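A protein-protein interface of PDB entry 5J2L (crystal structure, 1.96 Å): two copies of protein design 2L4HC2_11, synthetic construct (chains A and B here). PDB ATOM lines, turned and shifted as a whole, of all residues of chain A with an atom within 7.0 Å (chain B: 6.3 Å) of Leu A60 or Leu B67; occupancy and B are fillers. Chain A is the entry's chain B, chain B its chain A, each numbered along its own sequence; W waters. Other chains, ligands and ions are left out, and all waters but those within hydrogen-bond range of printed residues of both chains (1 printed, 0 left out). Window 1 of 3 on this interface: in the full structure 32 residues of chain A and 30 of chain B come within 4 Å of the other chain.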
ATOM      1  N   GLN A  21      -0.225  21.183 -21.506  1.00  0.00           N
ATOM      2  CA  GLN A  21       0.443  21.806 -20.380  1.00  0.00           C
ATOM      3  C   GLN A  21       0.025  21.160 -19.083  1.00  0.00           C
ATOM      4  O   GLN A  21       0.865  20.977 -18.205  1.00  0.00           O
ATOM      5  CB  GLN A  21       0.188  23.312 -20.335  1.00  0.00           C
ATOM      6  CG  GLN A  21       0.824  24.067 -21.483  1.00  0.00           C
ATOM      7  CD  GLN A  21       2.312  23.772 -21.580  1.00  0.00           C
ATOM      8  OE1 GLN A  21       2.992  23.571 -20.565  1.00  0.00           O
ATOM      9  NE2 GLN A  21       2.830  23.728 -22.804  1.00  0.00           N
ATOM     10  N   THR A  25       2.647  19.608 -16.437  1.00  0.00           N
ATOM     11  CA  THR A  25       2.666  19.968 -15.013  1.00  0.00           C
ATOM     12  C   THR A  25       2.680  18.724 -14.148  1.00  0.00           C
ATOM     13  O   THR A  25       3.412  18.665 -13.160  1.00  0.00           O
ATOM     14  CB  THR A  25       1.476  20.854 -14.604  1.00  0.00           C
ATOM     15  OG1 THR A  25       1.526  22.104 -15.299  1.00  0.00           O
ATOM     16  CG2 THR A  25       1.510  21.117 -13.105  1.00  0.00           C
ATOM     17  N   ILE A  28       6.127  17.241 -14.140  1.00  0.00           N
ATOM     18  CA  ILE A  28       7.032  18.022 -13.301  1.00  0.00           C
ATOM     19  C   ILE A  28       6.820  17.701 -11.832  1.00  0.00           C
ATOM     20  O   ILE A  28       7.785  17.550 -11.083  1.00  0.00           O
ATOM     21  CB  ILE A  28       6.896  19.526 -13.581  1.00  0.00           C
ATOM     22  CG1 ILE A  28       7.458  19.811 -14.988  1.00  0.00           C
ATOM     23  CG2 ILE A  28       7.575  20.366 -12.500  1.00  0.00           C
ATOM     24  CD1 ILE A  28       7.137  21.185 -15.520  1.00  0.00           C
ATOM     25  N   LEU A  32       9.603  16.012  -9.325  1.00  0.00           N
ATOM     26  CA  LEU A  32      10.051  16.630  -8.080  1.00  0.00           C
ATOM     27  C   LEU A  32       9.900  15.660  -6.897  1.00  0.00           C
ATOM     28  O   LEU A  32      10.755  15.639  -6.009  1.00  0.00           O
ATOM     29  CB  LEU A  32       9.323  17.968  -7.855  1.00  0.00           C
ATOM     30  CG  LEU A  32       9.790  19.123  -8.780  1.00  0.00           C
ATOM     31  CD1 LEU A  32       8.833  20.301  -8.673  1.00  0.00           C
ATOM     32  CD2 LEU A  32      11.197  19.556  -8.353  1.00  0.00           C
ATOM     33  N   GLU A  55      17.304  20.585 -14.745  1.00  0.00           N
ATOM     34  CA  GLU A  55      16.373  20.156 -15.788  1.00  0.00           C
ATOM     35  C   GLU A  55      14.920  20.530 -15.452  1.00  0.00           C
ATOM     36  O   GLU A  55      14.180  20.968 -16.334  1.00  0.00           O
ATOM     37  CB  GLU A  55      16.551  18.660 -16.058  1.00  0.00           C
ATOM     38  CG  GLU A  55      15.594  18.051 -17.095  1.00  0.00           C
ATOM     39  CD  GLU A  55      15.677  18.656 -18.476  1.00  0.00           C
ATOM     40  OE1 GLU A  55      16.587  19.403 -18.754  1.00  0.00           O
ATOM     41  OE2 GLU A  55      14.815  18.353 -19.269  1.00  0.00           O
ATOM     42  N   ILE A  56      14.513  20.389 -14.187  1.00  0.00           N
ATOM     43  CA  ILE A  56      13.167  20.809 -13.805  1.00  0.00           C
ATOM     44  C   ILE A  56      12.979  22.284 -14.077  1.00  0.00           C
ATOM     45  O   ILE A  56      11.942  22.697 -14.584  1.00  0.00           O
ATOM     46  CB  ILE A  56      12.828  20.555 -12.312  1.00  0.00           C
ATOM     47  CG1 ILE A  56      12.788  19.067 -11.980  1.00  0.00           C
ATOM     48  CG2 ILE A  56      11.478  21.200 -11.996  1.00  0.00           C
ATOM     49  CD1 ILE A  56      11.705  18.311 -12.709  1.00  0.00           C
ATOM     50  N   ILE A  57      13.978  23.083 -13.747  1.00  0.00           N
ATOM     51  CA  ILE A  57      13.833  24.507 -13.958  1.00  0.00           C
ATOM     52  C   ILE A  57      13.646  24.808 -15.432  1.00  0.00           C
ATOM     53  O   ILE A  57      12.779  25.598 -15.800  1.00  0.00           O
ATOM     54  CB  ILE A  57      15.016  25.279 -13.353  1.00  0.00           C
ATOM     55  CG1 ILE A  57      14.947  25.181 -11.825  1.00  0.00           C
ATOM     56  CG2 ILE A  57      15.019  26.717 -13.822  1.00  0.00           C
ATOM     57  CD1 ILE A  57      16.199  25.661 -11.115  1.00  0.00           C
ATOM     58  N   ARG A  58      14.449  24.169 -16.266  1.00  0.00           N
ATOM     59  CA  ARG A  58      14.375  24.379 -17.696  1.00  0.00           C
ATOM     60  C   ARG A  58      12.944  24.090 -18.176  1.00  0.00           C
ATOM     61  O   ARG A  58      12.365  24.858 -18.947  1.00  0.00           O
ATOM     62  CB  ARG A  58      15.413  23.505 -18.406  1.00  0.00           C
ATOM     63  CG  ARG A  58      15.612  23.806 -19.880  1.00  0.00           C
ATOM     64  CD  ARG A  58      16.451  22.786 -20.550  1.00  0.00           C
ATOM     65  NE  ARG A  58      15.760  21.513 -20.566  1.00  0.00           N
ATOM     66  CZ  ARG A  58      14.719  21.244 -21.376  1.00  0.00           C
ATOM     67  NH1 ARG A  58      14.292  22.169 -22.209  1.00  0.00           N
ATOM     68  NH2 ARG A  58      14.123  20.067 -21.326  1.00  0.00           N
ATOM     69  N   ARG A  59      12.377  22.986 -17.697  1.00  0.00           N
ATOM     70  CA  ARG A  59      11.032  22.584 -18.047  1.00  0.00           C
ATOM     71  C   ARG A  59       9.993  23.616 -17.587  1.00  0.00           C
ATOM     72  O   ARG A  59       9.068  23.944 -18.327  1.00  0.00           O
ATOM     73  CB  ARG A  59      10.737  21.198 -17.466  1.00  0.00           C
ATOM     74  CG  ARG A  59      11.552  20.089 -18.121  1.00  0.00           C
ATOM     75  CD  ARG A  59      11.178  18.726 -17.660  1.00  0.00           C
ATOM     76  NE  ARG A  59       9.855  18.349 -18.125  1.00  0.00           N
ATOM     77  CZ  ARG A  59       9.246  17.180 -17.854  1.00  0.00           C
ATOM     78  NH1 ARG A  59       9.861  16.278 -17.117  1.00  0.00           N
ATOM     79  NH2 ARG A  59       8.039  16.947 -18.344  1.00  0.00           N
ATOM     80  N   LEU A  60      10.149  24.145 -16.381  1.00  0.00           N
ATOM     81  CA  LEU A  60       9.217  25.159 -15.909  1.00  0.00           C
ATOM     82  C   LEU A  60       9.302  26.402 -16.772  1.00  0.00           C
ATOM     83  O   LEU A  60       8.284  27.004 -17.092  1.00  0.00           O
ATOM     84  CB  LEU A  60       9.474  25.523 -14.428  1.00  0.00           C
ATOM     85  CG  LEU A  60       9.073  24.473 -13.392  1.00  0.00           C
ATOM     86  CD1 LEU A  60       9.578  24.904 -12.016  1.00  0.00           C
ATOM     87  CD2 LEU A  60       7.562  24.347 -13.379  1.00  0.00           C
ATOM     88  N   GLN A  61      10.519  26.777 -17.149  1.00  0.00           N
ATOM     89  CA  GLN A  61      10.729  27.954 -17.970  1.00  0.00           C
ATOM     90  C   GLN A  61      10.055  27.771 -19.325  1.00  0.00           C
ATOM     91  O   GLN A  61       9.432  28.696 -19.846  1.00  0.00           O
ATOM     92  CB  GLN A  61      12.215  28.223 -18.119  1.00  0.00           C
ATOM     93  CG  GLN A  61      12.889  28.669 -16.838  1.00  0.00           C
ATOM     94  CD  GLN A  61      14.387  28.838 -17.014  1.00  0.00           C
ATOM     95  OE1 GLN A  61      15.006  28.221 -17.888  1.00  0.00           O
ATOM     96  NE2 GLN A  61      14.987  29.678 -16.187  1.00  0.00           N
ATOM     97  N   GLU A  62      10.166  26.575 -19.881  1.00  0.00           N
ATOM     98  CA  GLU A  62       9.515  26.289 -21.149  1.00  0.00           C
ATOM     99  C   GLU A  62       8.000  26.372 -21.019  1.00  0.00           C
ATOM    100  O   GLU A  62       7.324  26.927 -21.889  1.00  0.00           O
ATOM    101  CB  GLU A  62       9.930  24.920 -21.689  1.00  0.00           C
ATOM    102  CG  GLU A  62      11.372  24.848 -22.172  1.00  0.00           C
ATOM    103  CD  GLU A  62      11.755  23.501 -22.731  1.00  0.00           C
ATOM    104  OE1 GLU A  62      11.088  22.530 -22.452  1.00  0.00           O
ATOM    105  OE2 GLU A  62      12.720  23.446 -23.459  1.00  0.00           O
ATOM    106  N   GLN A  63       7.466  25.834 -19.930  1.00  0.00           N
ATOM    107  CA  GLN A  63       6.032  25.878 -19.702  1.00  0.00           C
ATOM    108  C   GLN A  63       5.543  27.308 -19.624  1.00  0.00           C
ATOM    109  O   GLN A  63       4.539  27.668 -20.241  1.00  0.00           O
ATOM    110  CB  GLN A  63       5.641  25.082 -18.448  1.00  0.00           C
ATOM    111  CG  GLN A  63       4.153  25.109 -18.182  1.00  0.00           C
ATOM    112  CD  GLN A  63       3.715  24.138 -17.113  1.00  0.00           C
ATOM    113  OE1 GLN A  63       4.120  24.208 -15.945  1.00  0.00           O
ATOM    114  NE2 GLN A  63       2.868  23.205 -17.537  1.00  0.00           N
ATOM    115  N   SER A  64       6.263  28.098 -18.864  1.00  0.00           N
ATOM    116  CA  SER A  64       5.993  29.492 -18.647  1.00  0.00           C
ATOM    117  C   SER A  64       5.926  30.252 -19.976  1.00  0.00           C
ATOM    118  O   SER A  64       4.978  30.999 -20.214  1.00  0.00           O
ATOM    119  CB  SER A  64       7.057  30.045 -17.726  1.00  0.00           C
ATOM    120  OG  SER A  64       6.870  31.400 -17.483  1.00  0.00           O
ATOM    121  N   GLU A  65       6.913  30.028 -20.842  1.00  0.00           N
ATOM    122  CA  GLU A  65       6.936  30.715 -22.133  1.00  0.00           C
ATOM    123  C   GLU A  65       5.760  30.300 -23.003  1.00  0.00           C
ATOM    124  O   GLU A  65       5.169  31.147 -23.673  1.00  0.00           O
ATOM    125  CB  GLU A  65       8.256  30.483 -22.841  1.00  0.00           C
ATOM    126  CG  GLU A  65       9.426  31.171 -22.150  1.00  0.00           C
ATOM    127  CD  GLU A  65       9.237  32.669 -22.053  1.00  0.00           C
ATOM    128  OE1 GLU A  65       8.871  33.270 -23.038  1.00  0.00           O
ATOM    129  OE2 GLU A  65       9.451  33.211 -20.990  1.00  0.00           O
ATOM    130  N   LYS A  66       5.365  29.028 -22.950  1.00  0.00           N
ATOM    131  CA  LYS A  66       4.206  28.614 -23.721  1.00  0.00           C
ATOM    132  C   LYS A  66       2.938  29.246 -23.198  1.00  0.00           C
ATOM    133  O   LYS A  66       2.076  29.639 -23.985  1.00  0.00           O
ATOM    134  CB  LYS A  66       4.077  27.092 -23.782  1.00  0.00           C
ATOM    135  CG  LYS A  66       5.058  26.469 -24.758  1.00  0.00           C
ATOM    136  CD  LYS A  66       4.679  26.900 -26.174  1.00  0.00           C
ATOM    137  CE  LYS A  66       5.695  26.469 -27.222  1.00  0.00           C
ATOM    138  NZ  LYS A  66       5.327  26.994 -28.576  1.00  0.00           N
ATOM    139  N   LEU A  67       2.830  29.391 -21.883  1.00  0.00           N
ATOM    140  CA  LEU A  67       1.635  30.012 -21.347  1.00  0.00           C
ATOM    141  C   LEU A  67       1.592  31.479 -21.748  1.00  0.00           C
ATOM    142  O   LEU A  67       0.516  32.016 -22.004  1.00  0.00           O
ATOM    143  CB  LEU A  67       1.565  29.864 -19.820  1.00  0.00           C
ATOM    144  CG  LEU A  67       1.374  28.434 -19.332  1.00  0.00           C
ATOM    145  CD1 LEU A  67       1.341  28.418 -17.806  1.00  0.00           C
ATOM    146  CD2 LEU A  67       0.116  27.863 -19.960  1.00  0.00           C
ATOM    147  N   LEU B  18       1.853  35.072 -13.925  1.00  0.00           N
ATOM    148  CA  LEU B  18       2.874  34.417 -14.718  1.00  0.00           C
ATOM    149  C   LEU B  18       4.185  35.198 -14.567  1.00  0.00           C
ATOM    150  O   LEU B  18       5.249  34.602 -14.447  1.00  0.00           O
ATOM    151  CB  LEU B  18       2.461  34.323 -16.201  1.00  0.00           C
ATOM    152  CG  LEU B  18       3.384  33.479 -17.103  1.00  0.00           C
ATOM    153  CD1 LEU B  18       3.358  32.033 -16.616  1.00  0.00           C
ATOM    154  CD2 LEU B  18       2.931  33.568 -18.556  1.00  0.00           C
ATOM    155  N   GLN B  21       5.756  34.254 -11.279  1.00  0.00           N
ATOM    156  CA  GLN B  21       6.479  32.987 -11.167  1.00  0.00           C
ATOM    157  C   GLN B  21       7.724  33.001 -12.025  1.00  0.00           C
ATOM    158  O   GLN B  21       8.708  32.363 -11.667  1.00  0.00           O
ATOM    159  CB  GLN B  21       5.650  31.739 -11.507  1.00  0.00           C
ATOM    160  CG  GLN B  21       5.206  31.630 -12.924  1.00  0.00           C
ATOM    161  CD  GLN B  21       6.295  31.140 -13.873  1.00  0.00           C
ATOM    162  OE1 GLN B  21       7.230  30.381 -13.585  1.00  0.00           O
ATOM    163  NE2 GLN B  21       6.137  31.641 -15.079  1.00  0.00           N
ATOM    164  N   THR B  25      10.994  31.895 -10.211  1.00  0.00           N
ATOM    165  CA  THR B  25      11.728  30.752 -10.736  1.00  0.00           C
ATOM    166  C   THR B  25      13.168  31.139 -11.037  1.00  0.00           C
ATOM    167  O   THR B  25      14.089  30.369 -10.760  1.00  0.00           O
ATOM    168  CB  THR B  25      11.026  30.142 -11.981  1.00  0.00           C
ATOM    169  OG1 THR B  25       9.725  29.657 -11.609  1.00  0.00           O
ATOM    170  CG2 THR B  25      11.844  28.998 -12.559  1.00  0.00           C
ATOM    171  N   LEU B  60      10.407  24.829  -5.953  1.00  0.00           N
ATOM    172  CA  LEU B  60      10.007  24.447  -7.303  1.00  0.00           C
ATOM    173  C   LEU B  60       8.610  23.824  -7.310  1.00  0.00           C
ATOM    174  O   LEU B  60       7.837  24.047  -8.238  1.00  0.00           O
ATOM    175  CB  LEU B  60      11.040  23.514  -7.931  1.00  0.00           C
ATOM    176  CG  LEU B  60      12.390  24.170  -8.258  1.00  0.00           C
ATOM    177  CD1 LEU B  60      13.380  23.109  -8.730  1.00  0.00           C
ATOM    178  CD2 LEU B  60      12.172  25.236  -9.343  1.00  0.00           C
ATOM    179  N   GLN B  61       8.269  23.069  -6.277  1.00  0.00           N
ATOM    180  CA  GLN B  61       6.941  22.468  -6.216  1.00  0.00           C
ATOM    181  C   GLN B  61       5.906  23.580  -6.186  1.00  0.00           C
ATOM    182  O   GLN B  61       4.878  23.499  -6.856  1.00  0.00           O
ATOM    183  CB  GLN B  61       6.822  21.541  -5.015  1.00  0.00           C
ATOM    184  CG  GLN B  61       7.661  20.273  -5.155  1.00  0.00           C
ATOM    185  CD  GLN B  61       7.690  19.449  -3.893  1.00  0.00           C
ATOM    186  OE1 GLN B  61       7.882  19.997  -2.806  1.00  0.00           O
ATOM    187  NE2 GLN B  61       7.498  18.139  -4.024  1.00  0.00           N
ATOM    188  N   GLU B  62       6.202  24.624  -5.415  1.00  0.00           N
ATOM    189  CA  GLU B  62       5.352  25.800  -5.312  1.00  0.00           C
ATOM    190  C   GLU B  62       5.190  26.479  -6.675  1.00  0.00           C
ATOM    191  O   GLU B  62       4.075  26.813  -7.078  1.00  0.00           O
ATOM    192  CB  GLU B  62       5.920  26.743  -4.247  1.00  0.00           C
ATOM    193  CG  GLU B  62       5.129  28.007  -3.970  1.00  0.00           C
ATOM    194  CD  GLU B  62       5.735  28.824  -2.842  1.00  0.00           C
ATOM    195  OE1 GLU B  62       6.701  28.384  -2.259  1.00  0.00           O
ATOM    196  OE2 GLU B  62       5.226  29.889  -2.566  1.00  0.00           O
ATOM    197  N   GLN B  63       6.297  26.679  -7.389  1.00  0.00           N
ATOM    198  CA  GLN B  63       6.215  27.313  -8.690  1.00  0.00           C
ATOM    199  C   GLN B  63       5.395  26.458  -9.664  1.00  0.00           C
ATOM    200  O   GLN B  63       4.629  26.989 -10.471  1.00  0.00           O
ATOM    201  CB  GLN B  63       7.612  27.579  -9.232  1.00  0.00           C
ATOM    202  CG  GLN B  63       8.368  28.612  -8.420  1.00  0.00           C
ATOM    203  CD  GLN B  63       7.675  29.954  -8.401  1.00  0.00           C
ATOM    204  OE1 GLN B  63       7.257  30.475  -9.441  1.00  0.00           O
ATOM    205  NE2 GLN B  63       7.563  30.535  -7.212  1.00  0.00           N
ATOM    206  N   SER B  64       5.542  25.137  -9.567  1.00  0.00           N
ATOM    207  CA  SER B  64       4.814  24.218 -10.434  1.00  0.00           C
ATOM    208  C   SER B  64       3.317  24.385 -10.200  1.00  0.00           C
ATOM    209  O   SER B  64       2.523  24.430 -11.144  1.00  0.00           O
ATOM    210  CB  SER B  64       5.273  22.791 -10.200  1.00  0.00           C
ATOM    211  OG  SER B  64       4.626  21.911 -11.064  1.00  0.00           O
ATOM    212  N   GLU B  65       2.944  24.476  -8.931  1.00  0.00           N
ATOM    213  CA  GLU B  65       1.556  24.647  -8.552  1.00  0.00           C
ATOM    214  C   GLU B  65       1.004  25.974  -9.067  1.00  0.00           C
ATOM    215  O   GLU B  65      -0.141  26.047  -9.516  1.00  0.00           O
ATOM    216  CB  GLU B  65       1.426  24.505  -7.032  1.00  0.00           C
ATOM    217  CG  GLU B  65       1.702  23.074  -6.573  1.00  0.00           C
ATOM    218  CD  GLU B  65       1.561  22.840  -5.088  1.00  0.00           C
ATOM    219  OE1 GLU B  65       0.820  23.554  -4.449  1.00  0.00           O
ATOM    220  OE2 GLU B  65       2.202  21.936  -4.594  1.00  0.00           O
ATOM    221  N   LYS B  66       1.827  27.016  -9.034  1.00  0.00           N
ATOM    222  CA  LYS B  66       1.395  28.309  -9.533  1.00  0.00           C
ATOM    223  C   LYS B  66       1.049  28.187 -11.023  1.00  0.00           C
ATOM    224  O   LYS B  66       0.030  28.708 -11.481  1.00  0.00           O
ATOM    225  CB  LYS B  66       2.475  29.387  -9.267  1.00  0.00           C
ATOM    226  CG  LYS B  66       2.631  29.734  -7.790  1.00  0.00           C
ATOM    227  CD  LYS B  66       3.702  30.801  -7.517  1.00  0.00           C
ATOM    228  CE  LYS B  66       3.795  31.086  -6.003  1.00  0.00           C
ATOM    229  NZ  LYS B  66       4.813  32.118  -5.663  1.00  0.00           N
ATOM    230  N   LEU B  67       1.876  27.471 -11.764  1.00  0.00           N
ATOM    231  CA  LEU B  67       1.609  27.292 -13.186  1.00  0.00           C
ATOM    232  C   LEU B  67       0.327  26.489 -13.413  1.00  0.00           C
ATOM    233  O   LEU B  67      -0.426  26.798 -14.326  1.00  0.00           O
ATOM    234  CB  LEU B  67       2.803  26.640 -13.880  1.00  0.00           C
ATOM    235  CG  LEU B  67       4.033  27.535 -14.006  1.00  0.00           C
ATOM    236  CD1 LEU B  67       5.204  26.725 -14.531  1.00  0.00           C
ATOM    237  CD2 LEU B  67       3.711  28.682 -14.944  1.00  0.00           C
ATOM    238  N   ARG B  68       0.082  25.492 -12.574  1.00  0.00           N
ATOM    239  CA  ARG B  68      -1.129  24.682 -12.656  1.00  0.00           C
ATOM    240  C   ARG B  68      -2.358  25.567 -12.529  1.00  0.00           C
ATOM    241  O   ARG B  68      -3.345  25.392 -13.250  1.00  0.00           O
ATOM    242  CB  ARG B  68      -1.148  23.598 -11.580  1.00  0.00           C
ATOM    243  CG  ARG B  68      -2.323  22.630 -11.651  1.00  0.00           C
ATOM    244  CD  ARG B  68      -2.282  21.620 -10.551  1.00  0.00           C
ATOM    245  NE  ARG B  68      -2.458  22.231  -9.234  1.00  0.00           N
ATOM    246  CZ  ARG B  68      -2.015  21.703  -8.071  1.00  0.00           C
ATOM    247  NH1 ARG B  68      -1.374  20.555  -8.066  1.00  0.00           N
ATOM    248  NH2 ARG B  68      -2.220  22.339  -6.930  1.00  0.00           N
ATOM    249  N   GLU B  69      -2.300  26.495 -11.576  1.00  0.00           N
ATOM    250  CA  GLU B  69      -3.400  27.411 -11.321  1.00  0.00           C
ATOM    251  C   GLU B  69      -3.644  28.351 -12.495  1.00  0.00           C
ATOM    252  O   GLU B  69      -4.799  28.613 -12.847  1.00  0.00           O
ATOM    253  CB  GLU B  69      -3.143  28.211 -10.042  1.00  0.00           C
ATOM    254  CG  GLU B  69      -3.188  27.358  -8.780  1.00  0.00           C
ATOM    255  CD  GLU B  69      -3.011  28.137  -7.501  1.00  0.00           C
ATOM    256  OE1 GLU B  69      -2.816  29.329  -7.557  1.00  0.00           O
ATOM    257  OE2 GLU B  69      -3.083  27.526  -6.460  1.00  0.00           O
ATOM    258  N   ILE B  70      -2.569  28.852 -13.101  1.00  0.00           N
ATOM    259  CA  ILE B  70      -2.688  29.717 -14.263  1.00  0.00           C
ATOM    260  C   ILE B  70      -3.364  28.970 -15.404  1.00  0.00           C
ATOM    261  O   ILE B  70      -4.260  29.496 -16.057  1.00  0.00           O
ATOM    262  CB  ILE B  70      -1.331  30.294 -14.685  1.00  0.00           C
ATOM    263  CG1 ILE B  70      -0.831  31.249 -13.597  1.00  0.00           C
ATOM    264  CG2 ILE B  70      -1.464  31.001 -16.018  1.00  0.00           C
ATOM    265  CD1 ILE B  70       0.615  31.657 -13.750  1.00  0.00           C
ATOM    266  N   ILE B  71      -2.931  27.728 -15.622  1.00  0.00           N
ATOM    267  CA  ILE B  71      -3.522  26.885 -16.667  1.00  0.00           C
ATOM    268  C   ILE B  71      -5.028  26.723 -16.426  1.00  0.00           C
ATOM    269  O   ILE B  71      -5.840  26.844 -17.354  1.00  0.00           O
ATOM    270  CB  ILE B  71      -2.828  25.497 -16.715  1.00  0.00           C
ATOM    271  CG1 ILE B  71      -1.403  25.651 -17.210  1.00  0.00           C
ATOM    272  CG2 ILE B  71      -3.592  24.539 -17.610  1.00  0.00           C
ATOM    273  CD1 ILE B  71      -0.565  24.420 -17.017  1.00  0.00           C
ATOM    274  N   GLU B  72      -5.391  26.455 -15.179  1.00  0.00           N
ATOM    275  CA  GLU B  72      -6.788  26.252 -14.811  1.00  0.00           C
ATOM    276  C   GLU B  72      -7.612  27.486 -15.147  1.00  0.00           C
ATOM    277  O   GLU B  72      -8.725  27.387 -15.673  1.00  0.00           O
ATOM    278  CB  GLU B  72      -6.899  25.917 -13.320  1.00  0.00           C
ATOM    279  CG  GLU B  72      -8.307  25.581 -12.842  1.00  0.00           C
ATOM    280  CD  GLU B  72      -8.783  24.249 -13.372  1.00  0.00           C
ATOM    281  OE1 GLU B  72      -7.956  23.473 -13.789  1.00  0.00           O
ATOM    282  OE2 GLU B  72      -9.966  23.995 -13.344  1.00  0.00           O
HETATM  283  O   HOH W   1       3.663  23.137 -13.584  1.00  0.00           O
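The side-chain hydroxyl of Thr A25 sits at hydrogen-bond distance from the backbone carbonyl oxygen of Gln A21, 3.2 Å away.
OE1 of Gln A21 sits at hydrogen-bond distance from NE2 of Gln A63, 3.1 Å away.
NE2 of Gln A63 lies within hydrogen-bond range of OG1 of Thr A25, at 2.8 Å.
The backbone carbonyl oxygen (O) of Leu B18 sits at hydrogen-bond distance from the side-chain amide nitrogen (NE2) of Gln B21, at 3.2 Å.
The side-chain hydroxyl of Thr B25 is in hydrogen-bond range of the backbone carbonyl oxygen of Gln B21 (2.9 Å).
The backbone carbonyl oxygen (O) of Gln B21 sits close to the side-chain amide oxygen (OE1) of Gln B63, at 3.3 Å.
Water W1 lies within hydrogen-bond range of the side-chain amide oxygen (OE1) of Gln A63 (2.6 Å), the side-chain hydroxyl (OG1) of Thr A25 (2.9 Å) and the side-chain hydroxyl (OG) of Ser B64 (3.0 Å).
Thr A25 touches Ser B64, but with the chains exchanged Ser A64 does not touch Thr B25 (6.7 Å).
Leu A60 touches Leu B67, but with the chains exchanged Leu A67 does not touch Leu B60 (12.4 Å).
Ser A64 touches Gln B21, but with the chains exchanged Gln A21 does not touch Ser B64 (8.0 Å).
Leu A67 touches its own counterpart, Leu B67.
Of the 16 pairs that touch across the chains among the printed residues, 2 have their exchanged pair printed and touching as well.
Printed residues of chain B within 4 Å of Ile A28: Ser B64 (3.6 Å).
Of chain B, only Leu B60 and Leu B67 come within 4 Å of Leu A60.
Printed residues of chain A within 4 Å of Gln B21: Ser A64.
Of the printed residues of chain A, Gln B61 touches Leu A32 (3.7 Å).
Printed residues of chain A within 4 Å of Ser B64: Thr A25 (3.8 Å) and Ile A28 (3.6 Å).
Leu B67 touches just these residues of chain A: Leu A60 (3.5 Å), Gln A63 (3.1 Å) and Leu A67 (3.7 Å).
Ile B70 touches none of the printed residues of chain A.
The nearest residue of chain B that does not touch Leu A60 is Ser B64 (4.03 Å).
CB of Gln A21 touches CD1 of Ile B71, 3.6 Å away.
Thr A25 touches Arg B68.
Ile B71 touches Thr A25.
Ser B64 touches Ile A28 (OG to CG2, 3.6 Å).
Leu A32 touches Gln B61.
Leu A60 touches Leu B60.
Gln A63 touches Leu B67 (OE1 to CD1, 3.1 Å).
OG of Ser A64 touches CD1 of Leu B18, 3.7 Å away.
Leu A67 touches Leu B67 (CD1 to CD2, 3.7 Å).
Ile B71 touches Leu A67 (CG1 to CD2, 3.8 Å).
Hydrophobic or aromatic side chains of chain B that line the printed part of chain A: Leu B18, Leu B60, Leu B67 and Ile B71.
Of the 17 printed residues of chain A, 9 touch a printed residue of chain B.
Hydrophobic or aromatic side chains of chain A within 4 Å of the printed part of chain B: Ile A28, Leu A32, Ile A57, Leu A60 and Leu A67.
Among the printed residues, no Asp or Glu carboxylate lies within 4 Å of a Lys or Arg side-chain nitrogen of the other chain.
The side-chain amide nitrogen (NE2) of Gln B21 sits at hydrogen-bond distance from the side-chain hydroxyl (OG) of Ser A64.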
